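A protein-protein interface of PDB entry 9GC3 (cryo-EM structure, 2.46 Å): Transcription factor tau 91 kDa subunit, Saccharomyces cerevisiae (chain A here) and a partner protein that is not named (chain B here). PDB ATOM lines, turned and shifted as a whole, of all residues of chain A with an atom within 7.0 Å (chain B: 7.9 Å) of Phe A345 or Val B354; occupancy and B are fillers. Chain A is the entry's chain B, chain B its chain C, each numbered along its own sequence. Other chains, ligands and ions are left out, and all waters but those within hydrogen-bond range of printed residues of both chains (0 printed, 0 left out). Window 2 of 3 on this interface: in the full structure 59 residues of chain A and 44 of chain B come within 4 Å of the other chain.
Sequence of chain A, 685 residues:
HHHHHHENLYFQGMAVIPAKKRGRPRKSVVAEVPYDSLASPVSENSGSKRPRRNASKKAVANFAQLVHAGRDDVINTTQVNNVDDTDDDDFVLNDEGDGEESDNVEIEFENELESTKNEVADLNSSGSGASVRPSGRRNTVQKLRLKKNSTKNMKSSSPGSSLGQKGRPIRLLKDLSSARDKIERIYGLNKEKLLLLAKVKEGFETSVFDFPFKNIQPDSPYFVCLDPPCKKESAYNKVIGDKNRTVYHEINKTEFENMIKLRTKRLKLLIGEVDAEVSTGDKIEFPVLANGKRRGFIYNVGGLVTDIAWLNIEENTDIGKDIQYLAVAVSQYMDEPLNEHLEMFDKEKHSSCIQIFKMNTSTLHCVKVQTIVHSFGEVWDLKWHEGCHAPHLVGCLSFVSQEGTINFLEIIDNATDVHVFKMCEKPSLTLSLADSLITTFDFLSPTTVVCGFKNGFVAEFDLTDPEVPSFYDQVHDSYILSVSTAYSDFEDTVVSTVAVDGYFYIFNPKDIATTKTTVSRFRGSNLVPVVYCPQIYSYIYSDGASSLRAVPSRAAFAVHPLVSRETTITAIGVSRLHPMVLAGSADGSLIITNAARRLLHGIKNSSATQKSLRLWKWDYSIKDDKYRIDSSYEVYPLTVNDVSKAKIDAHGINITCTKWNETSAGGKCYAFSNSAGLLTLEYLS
Printed residues of chain B that touch a printed residue of chain A: Val B354, Ala B355, Phe B356 and Lys B357.
Hydrophobic or aromatic side chains of chain A within 4 Å of the printed part of chain B: Phe A345 and Tyr A479.
Among the printed residues, pairs that only touch across the chains: Phe A345 with Val B354, Phe A345 with Ala B355, Phe A345 with Phe B356, Asp A477 with Lys B357, Ser A478 with Phe B356 and Tyr A479 with Phe B356.
The backbone NH (N) of Lys B357 lies within hydrogen-bond range of the side-chain hydroxyl (OG) of Ser A478.
The side-chain hydroxyl (OG) of Ser A478 is in hydrogen-bond range of the backbone carbonyl oxygen (O) of Ala B355 (2.7 Å).
Of the printed residues of chain A, Ala B355 touches Phe A345 and Ser A478.
Of the printed residues of chain A, Lys B357 touches Asp A477 and Ser A478.
Printed residues of chain B within 4 Å of Asp A477: Lys B357.
Of the printed residues of chain B, Tyr A479 touches Phe B356.
Printed residues of chain B within 4 Å of Ser A478: Ala B355, Phe B356 and Lys B357.
Asn B326 touches none of the printed residues of chain A.
The nearest residue of chain A that does not touch Val B354 is Lys A454 (4.2 Å).
The nearest printed residue of chain B that does not touch Ser A478 is Val B354 (6.4 Å).
The side-chain carboxylate (OE1) of Glu B352 is in salt-bridge range of the side-chain amino group (NZ) of Lys B357, 2.8 Å away.
O of Glu B328 sits at hydrogen-bond distance from N of Val B354 (2.9 Å).
O of Lys A454 sits close to N of Tyr A479 (3.4 Å).
The backbone carbonyl oxygen (O) of Arg B353 sits at hydrogen-bond distance from the side-chain amino group (NZ) of Lys B357 (2.9 Å).
The side-chain amino group (NZ) of Lys A454 lies within hydrogen-bond range of the backbone carbonyl oxygen (O) of Phe A345 (2.8 Å).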
ATOM      1  N   LEU A 342     -24.196  23.348 -12.161  1.00  0.00           N
ATOM      2  CA  LEU A 342     -22.930  23.231 -11.399  1.00  0.00           C
ATOM      3  C   LEU A 342     -23.169  23.483  -9.906  1.00  0.00           C
ATOM      4  O   LEU A 342     -22.178  23.540  -9.185  1.00  0.00           O
ATOM      5  CB  LEU A 342     -21.899  24.228 -11.915  1.00  0.00           C
ATOM      6  CG  LEU A 342     -21.448  24.028 -13.357  1.00  0.00           C
ATOM      7  CD1 LEU A 342     -20.366  25.051 -13.698  1.00  0.00           C
ATOM      8  CD2 LEU A 342     -20.964  22.617 -13.591  1.00  0.00           C
ATOM      9  N   GLU A 343     -24.404  23.604  -9.426  1.00  0.00           N
ATOM     10  CA  GLU A 343     -24.659  24.018  -8.016  1.00  0.00           C
ATOM     11  C   GLU A 343     -23.929  23.055  -7.045  1.00  0.00           C
ATOM     12  O   GLU A 343     -23.937  21.804  -7.222  1.00  0.00           O
ATOM     13  CB  GLU A 343     -26.171  24.075  -7.735  1.00  0.00           C
ATOM     14  CG  GLU A 343     -26.835  22.691  -7.649  1.00  0.00           C
ATOM     15  CD  GLU A 343     -28.315  22.639  -7.349  1.00  0.00           C
ATOM     16  OE1 GLU A 343     -28.764  23.420  -6.476  1.00  0.00           O
ATOM     17  OE2 GLU A 343     -29.019  21.826  -8.008  1.00  0.00           O
ATOM     18  N   MET A 344     -23.370  23.613  -5.996  1.00  0.00           N
ATOM     19  CA  MET A 344     -22.644  22.944  -4.883  1.00  0.00           C
ATOM     20  C   MET A 344     -23.615  22.310  -3.872  1.00  0.00           C
ATOM     21  O   MET A 344     -23.288  21.269  -3.340  1.00  0.00           O
ATOM     22  CB  MET A 344     -21.923  24.130  -4.231  1.00  0.00           C
ATOM     23  CG  MET A 344     -20.875  23.934  -3.273  1.00  0.00           C
ATOM     24  SD  MET A 344     -19.947  25.517  -3.165  1.00  0.00           S
ATOM     25  CE  MET A 344     -18.870  25.153  -1.785  1.00  0.00           C
ATOM     26  N   PHE A 345     -24.745  22.942  -3.556  1.00  0.00           N
ATOM     27  CA  PHE A 345     -25.449  22.796  -2.266  1.00  0.00           C
ATOM     28  C   PHE A 345     -26.522  21.702  -2.300  1.00  0.00           C
ATOM     29  O   PHE A 345     -26.890  21.234  -1.204  1.00  0.00           O
ATOM     30  CB  PHE A 345     -26.098  24.120  -1.879  1.00  0.00           C
ATOM     31  CG  PHE A 345     -26.557  24.173  -0.451  1.00  0.00           C
ATOM     32  CD1 PHE A 345     -25.617  24.164   0.572  1.00  0.00           C
ATOM     33  CD2 PHE A 345     -27.909  24.189  -0.121  1.00  0.00           C
ATOM     34  CE1 PHE A 345     -26.012  24.196   1.903  1.00  0.00           C
ATOM     35  CE2 PHE A 345     -28.303  24.212   1.212  1.00  0.00           C
ATOM     36  CZ  PHE A 345     -27.354  24.218   2.221  1.00  0.00           C
ATOM     37  N   ASP A 346     -27.026  21.268  -3.447  1.00  0.00           N
ATOM     38  CA  ASP A 346     -28.069  20.216  -3.443  1.00  0.00           C
ATOM     39  C   ASP A 346     -27.757  19.131  -4.472  1.00  0.00           C
ATOM     40  O   ASP A 346     -26.939  19.362  -5.382  1.00  0.00           O
ATOM     41  CB  ASP A 346     -29.434  20.875  -3.632  1.00  0.00           C
ATOM     42  CG  ASP A 346     -30.629  20.057  -3.155  1.00  0.00           C
ATOM     43  OD1 ASP A 346     -30.438  18.924  -2.645  1.00  0.00           O
ATOM     44  OD2 ASP A 346     -31.760  20.570  -3.284  1.00  0.00           O
ATOM     45  N   LYS A 347     -28.383  17.975  -4.289  1.00  0.00           N
ATOM     46  CA  LYS A 347     -28.164  16.770  -5.111  1.00  0.00           C
ATOM     47  C   LYS A 347     -28.509  17.078  -6.566  1.00  0.00           C
ATOM     48  O   LYS A 347     -29.665  17.440  -6.849  1.00  0.00           O
ATOM     49  CB  LYS A 347     -28.990  15.622  -4.543  1.00  0.00           C
ATOM     50  CG  LYS A 347     -28.665  14.252  -5.103  1.00  0.00           C
ATOM     51  CD  LYS A 347     -29.619  13.206  -4.615  1.00  0.00           C
ATOM     52  CE  LYS A 347     -29.194  11.789  -4.931  1.00  0.00           C
ATOM     53  NZ  LYS A 347     -28.287  11.256  -3.883  1.00  0.00           N
ATOM     54  N   GLN A 402     -21.685  15.313  -7.564  1.00  0.00           N
ATOM     55  CA  GLN A 402     -22.888  16.109  -7.225  1.00  0.00           C
ATOM     56  C   GLN A 402     -24.024  15.211  -6.760  1.00  0.00           C
ATOM     57  O   GLN A 402     -24.931  15.743  -6.089  1.00  0.00           O
ATOM     58  CB  GLN A 402     -23.344  16.916  -8.424  1.00  0.00           C
ATOM     59  CG  GLN A 402     -22.481  18.150  -8.619  1.00  0.00           C
ATOM     60  CD  GLN A 402     -23.044  18.928  -9.780  1.00  0.00           C
ATOM     61  OE1 GLN A 402     -23.049  18.442 -10.908  1.00  0.00           O
ATOM     62  NE2 GLN A 402     -23.519  20.134  -9.518  1.00  0.00           N
ATOM     63  N   LEU A 437     -25.280  14.826   2.015  1.00  0.00           N
ATOM     64  CA  LEU A 437     -24.447  14.691   0.807  1.00  0.00           C
ATOM     65  C   LEU A 437     -22.978  14.787   1.195  1.00  0.00           C
ATOM     66  O   LEU A 437     -22.589  15.784   1.826  1.00  0.00           O
ATOM     67  CB  LEU A 437     -24.770  15.812  -0.178  1.00  0.00           C
ATOM     68  CG  LEU A 437     -26.203  15.895  -0.673  1.00  0.00           C
ATOM     69  CD1 LEU A 437     -26.254  16.961  -1.751  1.00  0.00           C
ATOM     70  CD2 LEU A 437     -26.725  14.565  -1.198  1.00  0.00           C
ATOM     71  N   LYS A 454     -22.083  18.226   3.400  1.00  0.00           N
ATOM     72  CA  LYS A 454     -22.823  19.496   3.212  1.00  0.00           C
ATOM     73  C   LYS A 454     -23.225  20.091   4.563  1.00  0.00           C
ATOM     74  O   LYS A 454     -23.217  21.307   4.662  1.00  0.00           O
ATOM     75  CB  LYS A 454     -24.048  19.195   2.350  1.00  0.00           C
ATOM     76  CG  LYS A 454     -25.156  20.229   2.366  1.00  0.00           C
ATOM     77  CD  LYS A 454     -26.400  19.702   1.682  1.00  0.00           C
ATOM     78  CE  LYS A 454     -27.525  20.694   1.753  1.00  0.00           C
ATOM     79  NZ  LYS A 454     -28.625  20.304   0.843  1.00  0.00           N
ATOM     80  N   ASN A 455     -23.591  19.292   5.553  1.00  0.00           N
ATOM     81  CA  ASN A 455     -24.104  19.818   6.846  1.00  0.00           C
ATOM     82  C   ASN A 455     -22.976  20.119   7.833  1.00  0.00           C
ATOM     83  O   ASN A 455     -23.296  20.573   8.953  1.00  0.00           O
ATOM     84  CB  ASN A 455     -25.092  18.852   7.467  1.00  0.00           C
ATOM     85  CG  ASN A 455     -24.532  17.485   7.738  1.00  0.00           C
ATOM     86  OD1 ASN A 455     -23.382  17.203   7.417  1.00  0.00           O
ATOM     87  ND2 ASN A 455     -25.331  16.645   8.365  1.00  0.00           N
ATOM     88  N   GLY A 456     -21.717  19.881   7.467  1.00  0.00           N
ATOM     89  CA  GLY A 456     -20.577  20.140   8.366  1.00  0.00           C
ATOM     90  C   GLY A 456     -20.211  18.938   9.207  1.00  0.00           C
ATOM     91  O   GLY A 456     -19.418  19.108  10.119  1.00  0.00           O
ATOM     92  N   ASP A 477     -19.778  24.279  11.051  1.00  0.00           N
ATOM     93  CA  ASP A 477     -21.132  24.874  11.045  1.00  0.00           C
ATOM     94  C   ASP A 477     -21.799  24.720   9.679  1.00  0.00           C
ATOM     95  O   ASP A 477     -23.033  24.926   9.624  1.00  0.00           O
ATOM     96  CB  ASP A 477     -21.093  26.328  11.512  1.00  0.00           C
ATOM     97  CG  ASP A 477     -22.404  26.741  12.169  1.00  0.00           C
ATOM     98  OD1 ASP A 477     -23.293  25.867  12.345  1.00  0.00           O
ATOM     99  OD2 ASP A 477     -22.546  27.942  12.486  1.00  0.00           O
ATOM    100  N   SER A 478     -21.035  24.456   8.624  1.00  0.00           N
ATOM    101  CA  SER A 478     -21.533  24.565   7.237  1.00  0.00           C
ATOM    102  C   SER A 478     -20.710  23.697   6.281  1.00  0.00           C
ATOM    103  O   SER A 478     -19.862  22.933   6.734  1.00  0.00           O
ATOM    104  CB  SER A 478     -21.508  26.030   6.841  1.00  0.00           C
ATOM    105  OG  SER A 478     -22.375  26.275   5.742  1.00  0.00           O
ATOM    106  N   TYR A 479     -20.995  23.808   5.002  1.00  0.00           N
ATOM    107  CA  TYR A 479     -20.487  22.972   3.898  1.00  0.00           C
ATOM    108  C   TYR A 479     -18.965  22.817   4.009  1.00  0.00           C
ATOM    109  O   TYR A 479     -18.228  23.830   3.982  1.00  0.00           O
ATOM    110  CB  TYR A 479     -20.899  23.626   2.579  1.00  0.00           C
ATOM    111  CG  TYR A 479     -20.574  22.881   1.321  1.00  0.00           C
ATOM    112  CD1 TYR A 479     -19.264  22.768   0.874  1.00  0.00           C
ATOM    113  CD2 TYR A 479     -21.585  22.342   0.538  1.00  0.00           C
ATOM    114  CE1 TYR A 479     -18.969  22.089  -0.296  1.00  0.00           C
ATOM    115  CE2 TYR A 479     -21.303  21.634  -0.620  1.00  0.00           C
ATOM    116  CZ  TYR A 479     -19.988  21.539  -1.056  1.00  0.00           C
ATOM    117  OH  TYR A 479     -19.666  20.863  -2.200  1.00  0.00           O
ATOM    118  N   LYS B 287     -32.505  14.949  16.218  1.00  0.00           N
ATOM    119  CA  LYS B 287     -33.644  14.652  15.322  1.00  0.00           C
ATOM    120  C   LYS B 287     -34.770  13.921  16.037  1.00  0.00           C
ATOM    121  O   LYS B 287     -35.929  14.178  15.678  1.00  0.00           O
ATOM    122  CB  LYS B 287     -33.138  13.880  14.108  1.00  0.00           C
ATOM    123  CG  LYS B 287     -32.351  14.768  13.155  1.00  0.00           C
ATOM    124  CD  LYS B 287     -31.941  14.109  11.866  1.00  0.00           C
ATOM    125  CE  LYS B 287     -31.213  15.069  10.947  1.00  0.00           C
ATOM    126  NZ  LYS B 287     -30.352  14.355   9.974  1.00  0.00           N
ATOM    127  N   TRP B 317     -40.557  28.213  16.191  1.00  0.00           N
ATOM    128  CA  TRP B 317     -39.362  28.689  15.460  1.00  0.00           C
ATOM    129  C   TRP B 317     -39.563  28.489  13.951  1.00  0.00           C
ATOM    130  O   TRP B 317     -39.218  29.393  13.168  1.00  0.00           O
ATOM    131  CB  TRP B 317     -38.115  27.981  15.969  1.00  0.00           C
ATOM    132  CG  TRP B 317     -36.866  28.414  15.283  1.00  0.00           C
ATOM    133  CD1 TRP B 317     -35.980  29.369  15.679  1.00  0.00           C
ATOM    134  CD2 TRP B 317     -36.344  27.867  14.066  1.00  0.00           C
ATOM    135  NE1 TRP B 317     -34.943  29.472  14.784  1.00  0.00           N
ATOM    136  CE2 TRP B 317     -35.148  28.564  13.786  1.00  0.00           C
ATOM    137  CE3 TRP B 317     -36.779  26.853  13.196  1.00  0.00           C
ATOM    138  CZ2 TRP B 317     -34.378  28.274  12.670  1.00  0.00           C
ATOM    139  CZ3 TRP B 317     -36.032  26.588  12.075  1.00  0.00           C
ATOM    140  CH2 TRP B 317     -34.852  27.291  11.823  1.00  0.00           C
ATOM    141  N   ASN B 326     -39.268  25.914   2.824  1.00  0.00           N
ATOM    142  CA  ASN B 326     -38.246  26.226   1.790  1.00  0.00           C
ATOM    143  C   ASN B 326     -36.851  25.755   2.230  1.00  0.00           C
ATOM    144  O   ASN B 326     -35.975  25.638   1.358  1.00  0.00           O
ATOM    145  CB  ASN B 326     -38.228  27.717   1.455  1.00  0.00           C
ATOM    146  CG  ASN B 326     -39.331  28.136   0.505  1.00  0.00           C
ATOM    147  OD1 ASN B 326     -39.936  27.304  -0.171  1.00  0.00           O
ATOM    148  ND2 ASN B 326     -39.588  29.434   0.432  1.00  0.00           N
ATOM    149  N   TYR B 327     -36.629  25.500   3.519  1.00  0.00           N
ATOM    150  CA  TYR B 327     -35.303  25.111   4.059  1.00  0.00           C
ATOM    151  C   TYR B 327     -35.358  23.771   4.774  1.00  0.00           C
ATOM    152  O   TYR B 327     -36.403  23.388   5.318  1.00  0.00           O
ATOM    153  CB  TYR B 327     -34.784  26.162   5.025  1.00  0.00           C
ATOM    154  CG  TYR B 327     -34.577  27.525   4.428  1.00  0.00           C
ATOM    155  CD1 TYR B 327     -33.347  27.888   3.921  1.00  0.00           C
ATOM    156  CD2 TYR B 327     -35.580  28.476   4.440  1.00  0.00           C
ATOM    157  CE1 TYR B 327     -33.116  29.163   3.429  1.00  0.00           C
ATOM    158  CE2 TYR B 327     -35.372  29.751   3.939  1.00  0.00           C
ATOM    159  CZ  TYR B 327     -34.136  30.097   3.425  1.00  0.00           C
ATOM    160  OH  TYR B 327     -33.931  31.349   2.911  1.00  0.00           O
ATOM    161  N   GLU B 328     -34.222  23.075   4.756  1.00  0.00           N
ATOM    162  CA  GLU B 328     -33.938  21.948   5.672  1.00  0.00           C
ATOM    163  C   GLU B 328     -33.524  22.542   7.019  1.00  0.00           C
ATOM    164  O   GLU B 328     -32.673  23.428   7.052  1.00  0.00           O
ATOM    165  CB  GLU B 328     -32.868  21.045   5.076  1.00  0.00           C
ATOM    166  CG  GLU B 328     -32.575  19.832   5.935  1.00  0.00           C
ATOM    167  CD  GLU B 328     -31.641  18.809   5.297  1.00  0.00           C
ATOM    168  OE1 GLU B 328     -30.734  19.215   4.530  1.00  0.00           O
ATOM    169  OE2 GLU B 328     -31.824  17.599   5.563  1.00  0.00           O
ATOM    170  N   THR B 329     -34.092  22.080   8.118  1.00  0.00           N
ATOM    171  CA  THR B 329     -33.883  22.717   9.439  1.00  0.00           C
ATOM    172  C   THR B 329     -33.630  21.642  10.482  1.00  0.00           C
ATOM    173  O   THR B 329     -34.133  20.494  10.330  1.00  0.00           O
ATOM    174  CB  THR B 329     -35.096  23.564   9.828  1.00  0.00           C
ATOM    175  OG1 THR B 329     -36.303  22.825   9.649  1.00  0.00           O
ATOM    176  CG2 THR B 329     -35.171  24.817   9.002  1.00  0.00           C
ATOM    177  N   THR B 330     -32.934  22.020  11.535  1.00  0.00           N
ATOM    178  CA  THR B 330     -32.571  21.064  12.588  1.00  0.00           C
ATOM    179  C   THR B 330     -32.572  21.760  13.929  1.00  0.00           C
ATOM    180  O   THR B 330     -32.202  22.937  14.024  1.00  0.00           O
ATOM    181  CB  THR B 330     -31.216  20.392  12.292  1.00  0.00           C
ATOM    182  OG1 THR B 330     -31.021  19.282  13.171  1.00  0.00           O
ATOM    183  CG2 THR B 330     -30.045  21.326  12.459  1.00  0.00           C
ATOM    184  N   MET B 351     -31.675  26.384  17.137  1.00  0.00           N
ATOM    185  CA  MET B 351     -32.369  25.898  15.935  1.00  0.00           C
ATOM    186  C   MET B 351     -31.787  26.592  14.720  1.00  0.00           C
ATOM    187  O   MET B 351     -31.560  27.810  14.757  1.00  0.00           O
ATOM    188  CB  MET B 351     -33.866  26.130  16.064  1.00  0.00           C
ATOM    189  CG  MET B 351     -34.462  25.225  17.112  1.00  0.00           C
ATOM    190  SD  MET B 351     -36.031  25.794  17.753  1.00  0.00           S
ATOM    191  CE  MET B 351     -36.438  24.428  18.832  1.00  0.00           C
ATOM    192  N   GLU B 352     -31.523  25.806  13.686  1.00  0.00           N
ATOM    193  CA  GLU B 352     -30.666  26.226  12.559  1.00  0.00           C
ATOM    194  C   GLU B 352     -31.329  25.849  11.254  1.00  0.00           C
ATOM    195  O   GLU B 352     -31.980  24.785  11.158  1.00  0.00           O
ATOM    196  CB  GLU B 352     -29.300  25.543  12.673  1.00  0.00           C
ATOM    197  CG  GLU B 352     -28.368  26.171  13.698  1.00  0.00           C
ATOM    198  CD  GLU B 352     -27.967  27.603  13.386  1.00  0.00           C
ATOM    199  OE1 GLU B 352     -28.140  28.035  12.206  1.00  0.00           O
ATOM    200  OE2 GLU B 352     -27.466  28.274  14.313  1.00  0.00           O
ATOM    201  N   ARG B 353     -31.151  26.689  10.245  1.00  0.00           N
ATOM    202  CA  ARG B 353     -31.296  26.255   8.829  1.00  0.00           C
ATOM    203  C   ARG B 353     -29.972  25.644   8.382  1.00  0.00           C
ATOM    204  O   ARG B 353     -28.924  26.219   8.651  1.00  0.00           O
ATOM    205  CB  ARG B 353     -31.717  27.415   7.928  1.00  0.00           C
ATOM    206  CG  ARG B 353     -33.107  27.933   8.253  1.00  0.00           C
ATOM    207  CD  ARG B 353     -33.602  29.045   7.358  1.00  0.00           C
ATOM    208  NE  ARG B 353     -32.919  30.300   7.598  1.00  0.00           N
ATOM    209  CZ  ARG B 353     -33.419  31.504   7.343  1.00  0.00           C
ATOM    210  NH1 ARG B 353     -32.680  32.574   7.594  1.00  0.00           N
ATOM    211  NH2 ARG B 353     -34.650  31.652   6.877  1.00  0.00           N
ATOM    212  N   VAL B 354     -30.026  24.531   7.673  1.00  0.00           N
ATOM    213  CA  VAL B 354     -28.862  24.013   6.905  1.00  0.00           C
ATOM    214  C   VAL B 354     -28.639  24.944   5.714  1.00  0.00           C
ATOM    215  O   VAL B 354     -29.473  24.930   4.788  1.00  0.00           O
ATOM    216  CB  VAL B 354     -29.097  22.569   6.438  1.00  0.00           C
ATOM    217  CG1 VAL B 354     -27.867  22.029   5.723  1.00  0.00           C
ATOM    218  CG2 VAL B 354     -29.469  21.690   7.619  1.00  0.00           C
ATOM    219  N   ALA B 355     -27.564  25.711   5.759  1.00  0.00           N
ATOM    220  CA  ALA B 355     -27.290  26.791   4.806  1.00  0.00           C
ATOM    221  C   ALA B 355     -25.802  27.095   4.748  1.00  0.00           C
ATOM    222  O   ALA B 355     -25.074  26.784   5.664  1.00  0.00           O
ATOM    223  CB  ALA B 355     -28.073  27.995   5.254  1.00  0.00           C
ATOM    224  N   PHE B 356     -25.353  27.710   3.677  1.00  0.00           N
ATOM    225  CA  PHE B 356     -24.036  28.376   3.676  1.00  0.00           C
ATOM    226  C   PHE B 356     -24.130  29.438   4.762  1.00  0.00           C
ATOM    227  O   PHE B 356     -25.110  30.201   4.797  1.00  0.00           O
ATOM    228  CB  PHE B 356     -23.690  28.979   2.320  1.00  0.00           C
ATOM    229  CG  PHE B 356     -23.569  27.991   1.202  1.00  0.00           C
ATOM    230  CD1 PHE B 356     -22.717  26.904   1.322  1.00  0.00           C
ATOM    231  CD2 PHE B 356     -24.260  28.173   0.013  1.00  0.00           C
ATOM    232  CE1 PHE B 356     -22.590  25.994   0.283  1.00  0.00           C
ATOM    233  CE2 PHE B 356     -24.167  27.234  -1.007  1.00  0.00           C
ATOM    234  CZ  PHE B 356     -23.306  26.164  -0.886  1.00  0.00           C
ATOM    235  N   LYS B 357     -23.130  29.502   5.614  1.00  0.00           N
ATOM    236  CA  LYS B 357     -23.238  30.227   6.889  1.00  0.00           C
ATOM    237  C   LYS B 357     -21.854  30.660   7.364  1.00  0.00           C
ATOM    238  O   LYS B 357     -20.882  29.895   7.223  1.00  0.00           O
ATOM    239  CB  LYS B 357     -23.872  29.206   7.804  1.00  0.00           C
ATOM    240  CG  LYS B 357     -24.255  29.675   9.165  1.00  0.00           C
ATOM    241  CD  LYS B 357     -24.578  28.480  10.054  1.00  0.00           C
ATOM    242  CE  LYS B 357     -25.694  27.578   9.566  1.00  0.00           C
ATOM    243  NZ  LYS B 357     -27.019  28.208   9.689  1.00  0.00           N
